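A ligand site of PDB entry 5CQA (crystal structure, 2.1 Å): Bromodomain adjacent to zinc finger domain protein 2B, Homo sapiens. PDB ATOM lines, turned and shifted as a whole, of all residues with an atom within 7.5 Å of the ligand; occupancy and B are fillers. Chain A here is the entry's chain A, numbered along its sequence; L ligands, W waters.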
ATOM      1  N   ALA A  31      32.722 -30.321 -13.089  1.00  0.00           N
ATOM      2  CA  ALA A  31      31.554 -29.457 -12.891  1.00  0.00           C
ATOM      3  C   ALA A  31      30.269 -30.209 -12.517  1.00  0.00           C
ATOM      4  O   ALA A  31      29.329 -29.599 -11.983  1.00  0.00           O
ATOM      5  CB  ALA A  31      31.315 -28.609 -14.151  1.00  0.00           C
ATOM      6  N   TRP A  32      30.232 -31.518 -12.776  1.00  0.00           N
ATOM      7  CA  TRP A  32      28.975 -32.271 -12.730  1.00  0.00           C
ATOM      8  C   TRP A  32      28.205 -32.213 -11.398  1.00  0.00           C
ATOM      9  O   TRP A  32      26.985 -32.266 -11.409  1.00  0.00           O
ATOM     10  CB  TRP A  32      29.213 -33.744 -13.144  1.00  0.00           C
ATOM     11  CG  TRP A  32      30.221 -34.471 -12.311  1.00  0.00           C
ATOM     12  CD1 TRP A  32      31.573 -34.565 -12.547  1.00  0.00           C
ATOM     13  CD2 TRP A  32      29.981 -35.202 -11.086  1.00  0.00           C
ATOM     14  NE1 TRP A  32      32.173 -35.293 -11.546  1.00  0.00           N
ATOM     15  CE2 TRP A  32      31.221 -35.686 -10.641  1.00  0.00           C
ATOM     16  CE3 TRP A  32      28.838 -35.467 -10.334  1.00  0.00           C
ATOM     17  CZ2 TRP A  32      31.352 -36.444  -9.468  1.00  0.00           C
ATOM     18  CZ3 TRP A  32      28.966 -36.233  -9.167  1.00  0.00           C
ATOM     19  CH2 TRP A  32      30.209 -36.704  -8.762  1.00  0.00           C
ATOM     20  N   PRO A  33      28.892 -32.088 -10.243  1.00  0.00           N
ATOM     21  CA  PRO A  33      28.020 -31.951  -9.061  1.00  0.00           C
ATOM     22  C   PRO A  33      27.307 -30.609  -8.955  1.00  0.00           C
ATOM     23  O   PRO A  33      26.439 -30.485  -8.070  1.00  0.00           O
ATOM     24  CB  PRO A  33      28.991 -32.110  -7.889  1.00  0.00           C
ATOM     25  CG  PRO A  33      30.246 -32.726  -8.477  1.00  0.00           C
ATOM     26  CD  PRO A  33      30.308 -32.208  -9.868  1.00  0.00           C
ATOM     27  N   PHE A  34      27.649 -29.651  -9.809  1.00  0.00           N
ATOM     28  CA  PHE A  34      27.235 -28.249  -9.622  1.00  0.00           C
ATOM     29  C   PHE A  34      26.341 -27.715 -10.734  1.00  0.00           C
ATOM     30  O   PHE A  34      25.930 -26.561 -10.686  1.00  0.00           O
ATOM     31  CB  PHE A  34      28.471 -27.360  -9.485  1.00  0.00           C
ATOM     32  CG  PHE A  34      29.496 -27.897  -8.533  1.00  0.00           C
ATOM     33  CD1 PHE A  34      29.231 -27.929  -7.163  1.00  0.00           C
ATOM     34  CD2 PHE A  34      30.714 -28.405  -8.997  1.00  0.00           C
ATOM     35  CE1 PHE A  34      30.170 -28.456  -6.269  1.00  0.00           C
ATOM     36  CE2 PHE A  34      31.659 -28.921  -8.106  1.00  0.00           C
ATOM     37  CZ  PHE A  34      31.383 -28.956  -6.743  1.00  0.00           C
ATOM     38  N   LEU A  35      26.067 -28.536 -11.735  1.00  0.00           N
ATOM     39  CA  LEU A  35      25.404 -28.080 -12.953  1.00  0.00           C
ATOM     40  C   LEU A  35      23.929 -27.737 -12.716  1.00  0.00           C
ATOM     41  O   LEU A  35      23.411 -26.818 -13.338  1.00  0.00           O
ATOM     42  CB  LEU A  35      25.528 -29.124 -14.071  1.00  0.00           C
ATOM     43  CG  LEU A  35      26.916 -29.362 -14.707  1.00  0.00           C
ATOM     44  CD1 LEU A  35      26.889 -30.528 -15.713  1.00  0.00           C
ATOM     45  CD2 LEU A  35      27.455 -28.112 -15.392  1.00  0.00           C
ATOM     46  N   LEU A  36      23.278 -28.452 -11.804  1.00  0.00           N
ATOM     47  CA  LEU A  36      21.849 -28.269 -11.581  1.00  0.00           C
ATOM     48  C   LEU A  36      21.595 -28.150 -10.104  1.00  0.00           C
ATOM     49  O   LEU A  36      22.462 -28.520  -9.307  1.00  0.00           O
ATOM     50  CB  LEU A  36      21.046 -29.426 -12.194  1.00  0.00           C
ATOM     51  CG  LEU A  36      21.007 -29.560 -13.728  1.00  0.00           C
ATOM     52  CD1 LEU A  36      20.297 -30.863 -14.144  1.00  0.00           C
ATOM     53  CD2 LEU A  36      20.326 -28.345 -14.378  1.00  0.00           C
ATOM     54  N   PRO A  37      20.419 -27.632  -9.713  1.00  0.00           N
ATOM     55  CA  PRO A  37      20.138 -27.580  -8.271  1.00  0.00           C
ATOM     56  C   PRO A  37      20.151 -28.982  -7.668  1.00  0.00           C
ATOM     57  O   PRO A  37      19.693 -29.929  -8.332  1.00  0.00           O
ATOM     58  CB  PRO A  37      18.736 -26.980  -8.207  1.00  0.00           C
ATOM     59  CG  PRO A  37      18.549 -26.275  -9.529  1.00  0.00           C
ATOM     60  CD  PRO A  37      19.321 -27.070 -10.515  1.00  0.00           C
ATOM     61  N   VAL A  38      20.691 -29.127  -6.465  1.00  0.00           N
ATOM     62  CA  VAL A  38      20.584 -30.379  -5.719  1.00  0.00           C
ATOM     63  C   VAL A  38      19.090 -30.681  -5.497  1.00  0.00           C
ATOM     64  O   VAL A  38      18.330 -29.780  -5.131  1.00  0.00           O
ATOM     65  CB  VAL A  38      21.330 -30.305  -4.357  1.00  0.00           C
ATOM     66  CG1 VAL A  38      21.027 -31.525  -3.512  1.00  0.00           C
ATOM     67  CG2 VAL A  38      22.844 -30.160  -4.566  1.00  0.00           C
ATOM     68  N   ASN A  39      18.682 -31.918  -5.767  1.00  0.00           N
ATOM     69  CA  ASN A  39      17.249 -32.282  -5.671  1.00  0.00           C
ATOM     70  C   ASN A  39      16.821 -32.377  -4.214  1.00  0.00           C
ATOM     71  O   ASN A  39      17.183 -33.333  -3.526  1.00  0.00           O
ATOM     72  CB  ASN A  39      16.968 -33.600  -6.411  1.00  0.00           C
ATOM     73  CG  ASN A  39      15.463 -33.917  -6.529  1.00  0.00           C
ATOM     74  OD1 ASN A  39      14.657 -33.566  -5.656  1.00  0.00           O
ATOM     75  ND2 ASN A  39      15.095 -34.572  -7.608  1.00  0.00           N
ATOM     76  N   LEU A  42      14.937 -35.542  -3.081  1.00  0.00           N
ATOM     77  CA  LEU A  42      15.649 -36.821  -3.130  1.00  0.00           C
ATOM     78  C   LEU A  42      16.896 -36.902  -2.241  1.00  0.00           C
ATOM     79  O   LEU A  42      17.446 -37.988  -2.057  1.00  0.00           O
ATOM     80  CB  LEU A  42      16.041 -37.147  -4.567  1.00  0.00           C
ATOM     81  CG  LEU A  42      14.890 -37.381  -5.552  1.00  0.00           C
ATOM     82  CD1 LEU A  42      15.435 -37.657  -6.942  1.00  0.00           C
ATOM     83  CD2 LEU A  42      14.009 -38.529  -5.066  1.00  0.00           C
ATOM     84  N   VAL A  43      17.347 -35.774  -1.706  1.00  0.00           N
ATOM     85  CA  VAL A  43      18.556 -35.773  -0.876  1.00  0.00           C
ATOM     86  C   VAL A  43      18.237 -35.372   0.560  1.00  0.00           C
ATOM     87  O   VAL A  43      18.124 -34.183   0.871  1.00  0.00           O
ATOM     88  CB  VAL A  43      19.619 -34.837  -1.450  1.00  0.00           C
ATOM     89  CG1 VAL A  43      20.908 -34.908  -0.634  1.00  0.00           C
ATOM     90  CG2 VAL A  43      19.894 -35.178  -2.912  1.00  0.00           C
ATOM     91  N   TYR A  46      19.372 -32.059   2.991  1.00  0.00           N
ATOM     92  CA  TYR A  46      19.866 -30.895   2.253  1.00  0.00           C
ATOM     93  C   TYR A  46      19.053 -29.632   2.491  1.00  0.00           C
ATOM     94  O   TYR A  46      19.621 -28.563   2.733  1.00  0.00           O
ATOM     95  CB  TYR A  46      19.941 -31.178   0.743  1.00  0.00           C
ATOM     96  CG  TYR A  46      21.002 -30.300   0.089  1.00  0.00           C
ATOM     97  CD1 TYR A  46      22.345 -30.684   0.075  1.00  0.00           C
ATOM     98  CD2 TYR A  46      20.663 -29.068  -0.458  1.00  0.00           C
ATOM     99  CE1 TYR A  46      23.313 -29.867  -0.495  1.00  0.00           C
ATOM    100  CE2 TYR A  46      21.632 -28.255  -1.041  1.00  0.00           C
ATOM    101  CZ  TYR A  46      22.951 -28.642  -1.055  1.00  0.00           C
ATOM    102  OH  TYR A  46      23.911 -27.821  -1.627  1.00  0.00           O
ATOM    103  N   ILE A  50      21.184 -26.640   4.272  1.00  0.00           N
ATOM    104  CA  ILE A  50      21.721 -25.642   3.346  1.00  0.00           C
ATOM    105  C   ILE A  50      20.714 -24.516   3.096  1.00  0.00           C
ATOM    106  O   ILE A  50      19.811 -24.651   2.276  1.00  0.00           O
ATOM    107  CB  ILE A  50      22.110 -26.315   2.006  1.00  0.00           C
ATOM    108  CG1 ILE A  50      23.120 -27.433   2.261  1.00  0.00           C
ATOM    109  CG2 ILE A  50      22.697 -25.284   1.023  1.00  0.00           C
ATOM    110  CD1 ILE A  50      24.469 -26.948   2.810  1.00  0.00           C
ATOM    111  N   MET A  54      22.623 -23.023  -4.215  1.00  0.00           N
ATOM    112  CA  MET A  54      23.075 -22.310  -5.402  1.00  0.00           C
ATOM    113  C   MET A  54      23.825 -23.296  -6.302  1.00  0.00           C
ATOM    114  O   MET A  54      24.445 -24.245  -5.820  1.00  0.00           O
ATOM    115  CB  MET A  54      23.955 -21.107  -5.008  1.00  0.00           C
ATOM    116  CG  MET A  54      24.318 -20.158  -6.174  1.00  0.00           C
ATOM    117  SD  MET A  54      22.899 -19.546  -7.131  1.00  0.00           S
ATOM    118  CE  MET A  54      21.959 -18.754  -5.811  1.00  0.00           C
ATOM    119  N   ASP A  55      23.742 -23.074  -7.609  1.00  0.00           N
ATOM    120  CA  ASP A  55      24.337 -23.955  -8.611  1.00  0.00           C
ATOM    121  C   ASP A  55      24.564 -23.154  -9.877  1.00  0.00           C
ATOM    122  O   ASP A  55      24.011 -22.053 -10.006  1.00  0.00           O
ATOM    123  CB  ASP A  55      23.403 -25.140  -8.910  1.00  0.00           C
ATOM    124  CG  ASP A  55      22.190 -24.709  -9.698  1.00  0.00           C
ATOM    125  OD1 ASP A  55      21.253 -24.134  -9.096  1.00  0.00           O
ATOM    126  OD2 ASP A  55      22.169 -24.914 -10.920  1.00  0.00           O
ATOM    127  N   VAL A  81      28.364 -21.593  -3.938  1.00  0.00           N
ATOM    128  CA  VAL A  81      28.275 -22.963  -4.447  1.00  0.00           C
ATOM    129  C   VAL A  81      29.277 -23.883  -3.740  1.00  0.00           C
ATOM    130  O   VAL A  81      28.950 -25.002  -3.341  1.00  0.00           O
ATOM    131  CB  VAL A  81      28.526 -23.019  -5.978  1.00  0.00           C
ATOM    132  CG1 VAL A  81      28.683 -24.481  -6.472  1.00  0.00           C
ATOM    133  CG2 VAL A  81      27.412 -22.311  -6.724  1.00  0.00           C
ATOM    134  N   PHE A  82      30.498 -23.390  -3.574  1.00  0.00           N
ATOM    135  CA  PHE A  82      31.573 -24.235  -3.050  1.00  0.00           C
ATOM    136  C   PHE A  82      31.570 -24.275  -1.517  1.00  0.00           C
ATOM    137  O   PHE A  82      31.920 -25.288  -0.925  1.00  0.00           O
ATOM    138  CB  PHE A  82      32.930 -23.747  -3.614  1.00  0.00           C
ATOM    139  CG  PHE A  82      32.949 -23.697  -5.134  1.00  0.00           C
ATOM    140  CD1 PHE A  82      32.511 -24.788  -5.876  1.00  0.00           C
ATOM    141  CD2 PHE A  82      33.362 -22.553  -5.799  1.00  0.00           C
ATOM    142  CE1 PHE A  82      32.487 -24.749  -7.264  1.00  0.00           C
ATOM    143  CE2 PHE A  82      33.357 -22.502  -7.196  1.00  0.00           C
ATOM    144  CZ  PHE A  82      32.912 -23.605  -7.935  1.00  0.00           C
ATOM    145  N   ASN A  84      28.644 -24.164   0.163  1.00  0.00           N
ATOM    146  CA  ASN A  84      27.616 -25.189   0.367  1.00  0.00           C
ATOM    147  C   ASN A  84      28.195 -26.594   0.204  1.00  0.00           C
ATOM    148  O   ASN A  84      27.881 -27.476   0.988  1.00  0.00           O
ATOM    149  CB  ASN A  84      26.457 -25.011  -0.602  1.00  0.00           C
ATOM    150  CG  ASN A  84      25.610 -23.786  -0.290  1.00  0.00           C
ATOM    151  OD1 ASN A  84      25.737 -23.203   0.787  1.00  0.00           O
ATOM    152  ND2 ASN A  84      24.732 -23.402  -1.230  1.00  0.00           N
ATOM    153  N   CYS A  85      29.035 -26.773  -0.808  1.00  0.00           N
ATOM    154  CA  CYS A  85      29.601 -28.091  -1.089  1.00  0.00           C
ATOM    155  C   CYS A  85      30.395 -28.605   0.122  1.00  0.00           C
ATOM    156  O   CYS A  85      30.250 -29.769   0.522  1.00  0.00           O
ATOM    157  CB  CYS A  85      30.477 -28.062  -2.329  1.00  0.00           C
ATOM    158  SG  CYS A  85      31.164 -29.670  -2.828  1.00  0.00           S
ATOM    159  N   GLU A  86      31.210 -27.726   0.707  1.00  0.00           N
ATOM    160  CA  GLU A  86      32.038 -28.080   1.871  1.00  0.00           C
ATOM    161  C   GLU A  86      31.230 -28.402   3.110  1.00  0.00           C
ATOM    162  O   GLU A  86      31.624 -29.225   3.919  1.00  0.00           O
ATOM    163  CB  GLU A  86      32.995 -26.947   2.213  1.00  0.00           C
ATOM    164  CG  GLU A  86      34.120 -26.795   1.249  1.00  0.00           C
ATOM    165  CD  GLU A  86      35.303 -26.091   1.885  1.00  0.00           C
ATOM    166  OE1 GLU A  86      35.618 -26.398   3.059  1.00  0.00           O
ATOM    167  OE2 GLU A  86      35.891 -25.215   1.198  1.00  0.00           O
ATOM    168  N   PHE A  88      28.289 -29.836   3.240  1.00  0.00           N
ATOM    169  CA  PHE A  88      27.515 -31.052   3.156  1.00  0.00           C
ATOM    170  C   PHE A  88      28.328 -32.294   2.795  1.00  0.00           C
ATOM    171  O   PHE A  88      27.841 -33.418   2.938  1.00  0.00           O
ATOM    172  CB  PHE A  88      26.387 -30.852   2.140  1.00  0.00           C
ATOM    173  CG  PHE A  88      25.213 -31.793   2.321  1.00  0.00           C
ATOM    174  CD1 PHE A  88      24.241 -31.516   3.262  1.00  0.00           C
ATOM    175  CD2 PHE A  88      25.071 -32.905   1.521  1.00  0.00           C
ATOM    176  CE1 PHE A  88      23.149 -32.353   3.413  1.00  0.00           C
ATOM    177  CE2 PHE A  88      23.976 -33.750   1.666  1.00  0.00           C
ATOM    178  CZ  PHE A  88      23.013 -33.474   2.623  1.00  0.00           C
ATOM    179  N   ASN A  89      29.545 -32.102   2.294  1.00  0.00           N
ATOM    180  CA  ASN A  89      30.327 -33.205   1.748  1.00  0.00           C
ATOM    181  C   ASN A  89      31.669 -33.347   2.454  1.00  0.00           C
ATOM    182  O   ASN A  89      32.335 -32.353   2.751  1.00  0.00           O
ATOM    183  CB  ASN A  89      30.556 -33.003   0.244  1.00  0.00           C
ATOM    184  CG  ASN A  89      29.273 -33.034  -0.574  1.00  0.00           C
ATOM    185  OD1 ASN A  89      28.817 -34.109  -0.999  1.00  0.00           O
ATOM    186  ND2 ASN A  89      28.668 -31.867  -0.789  1.00  0.00           N
ATOM    187  N   ILE A  95      32.726 -35.690  -4.552  1.00  0.00           N
ATOM    188  CA  ILE A  95      32.079 -34.379  -4.639  1.00  0.00           C
ATOM    189  C   ILE A  95      32.868 -33.336  -3.836  1.00  0.00           C
ATOM    190  O   ILE A  95      33.073 -32.213  -4.301  1.00  0.00           O
ATOM    191  CB  ILE A  95      30.615 -34.414  -4.156  1.00  0.00           C
ATOM    192  CG1 ILE A  95      29.777 -35.274  -5.105  1.00  0.00           C
ATOM    193  CG2 ILE A  95      30.023 -32.984  -4.095  1.00  0.00           C
ATOM    194  CD1 ILE A  95      28.307 -35.440  -4.705  1.00  0.00           C
ATOM    195  N   GLY A  96      33.334 -33.726  -2.660  1.00  0.00           N
ATOM    196  CA  GLY A  96      34.212 -32.890  -1.864  1.00  0.00           C
ATOM    197  C   GLY A  96      35.456 -32.424  -2.611  1.00  0.00           C
ATOM    198  O   GLY A  96      35.791 -31.244  -2.587  1.00  0.00           O
ATOM    199  N   GLY A  99      34.620 -29.964  -5.455  1.00  0.00           N
ATOM    200  CA  GLY A  99      34.373 -28.629  -4.948  1.00  0.00           C
ATOM    201  C   GLY A  99      35.656 -27.829  -4.763  1.00  0.00           C
ATOM    202  O   GLY A  99      35.758 -26.679  -5.212  1.00  0.00           O
HETATM  203  C1  LIG L   1      27.328 -29.922  -4.822  1.00  0.00           C
HETATM  204  N1  LIG L   1      26.549 -31.149  -4.793  1.00  0.00           N
HETATM  205  C2  LIG L   1      26.178 -31.717  -3.641  1.00  0.00           C
HETATM  206  C3  LIG L   1      25.369 -32.942  -3.746  1.00  0.00           C
HETATM  207  C4  LIG L   1      25.011 -33.669  -4.893  1.00  0.00           C
HETATM  208  C5  LIG L   1      24.216 -34.784  -4.595  1.00  0.00           C
HETATM  209  C6  LIG L   1      23.963 -34.934  -3.244  1.00  0.00           C
HETATM  210  S1  LIG L   1      24.702 -33.678  -2.390  1.00  0.00           S
HETATM  211  O1  LIG L   1      23.736 -35.694  -5.650  1.00  0.00           O
HETATM  212  C7  LIG L   1      24.493 -35.486  -6.862  1.00  0.00           C
HETATM  213  C8  LIG L   1      24.586 -34.028  -7.217  1.00  0.00           C
HETATM  214  O2  LIG L   1      25.398 -33.310  -6.269  1.00  0.00           O
HETATM  215  O3  LIG L   1      26.501 -31.253  -2.536  1.00  0.00           O
HETATM  216  O   HOH W   1      26.988 -26.773  -3.997  1.00  0.00           O
HETATM  217  O   HOH W   2      26.356 -28.753  -2.021  1.00  0.00           O
HETATM  218  O   HOH W   3      22.668 -31.952  -8.930  1.00  0.00           O
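The side-chain amide nitrogen (ND2) of Asn 89 lies within hydrogen-bond range of the backbone carbonyl oxygen (O) of Cys 85, 2.9 Å away.
The side-chain sulfur (SG) of Cys 85 is in hydrogen-bond range of the backbone carbonyl oxygen (O) of Ile 95, 3.5 Å away.
The backbone carbonyl oxygen (O) of Pro 33 lies within hydrogen-bond range of a nitrogen (N1) of the ligand (3.3 Å).
ND2 of Asn 89 is in hydrogen-bond range of O3 of the ligand (2.9 Å).
Water W2 bridges an oxygen (O3) of the ligand (2.6 Å) and the side-chain hydroxyl of Tyr 46 (2.6 Å).
Phe 34 touches the ligand.
Val 38 touches the ligand (CG2 to C2, 3.8 Å).
Ile 95 touches the ligand.
Hydrophobic or aromatic side chains that line the ligand: Phe 34, Val 38 and Ile 95.
Of the 25 residues printed, 5 come within 4 Å of the ligand.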
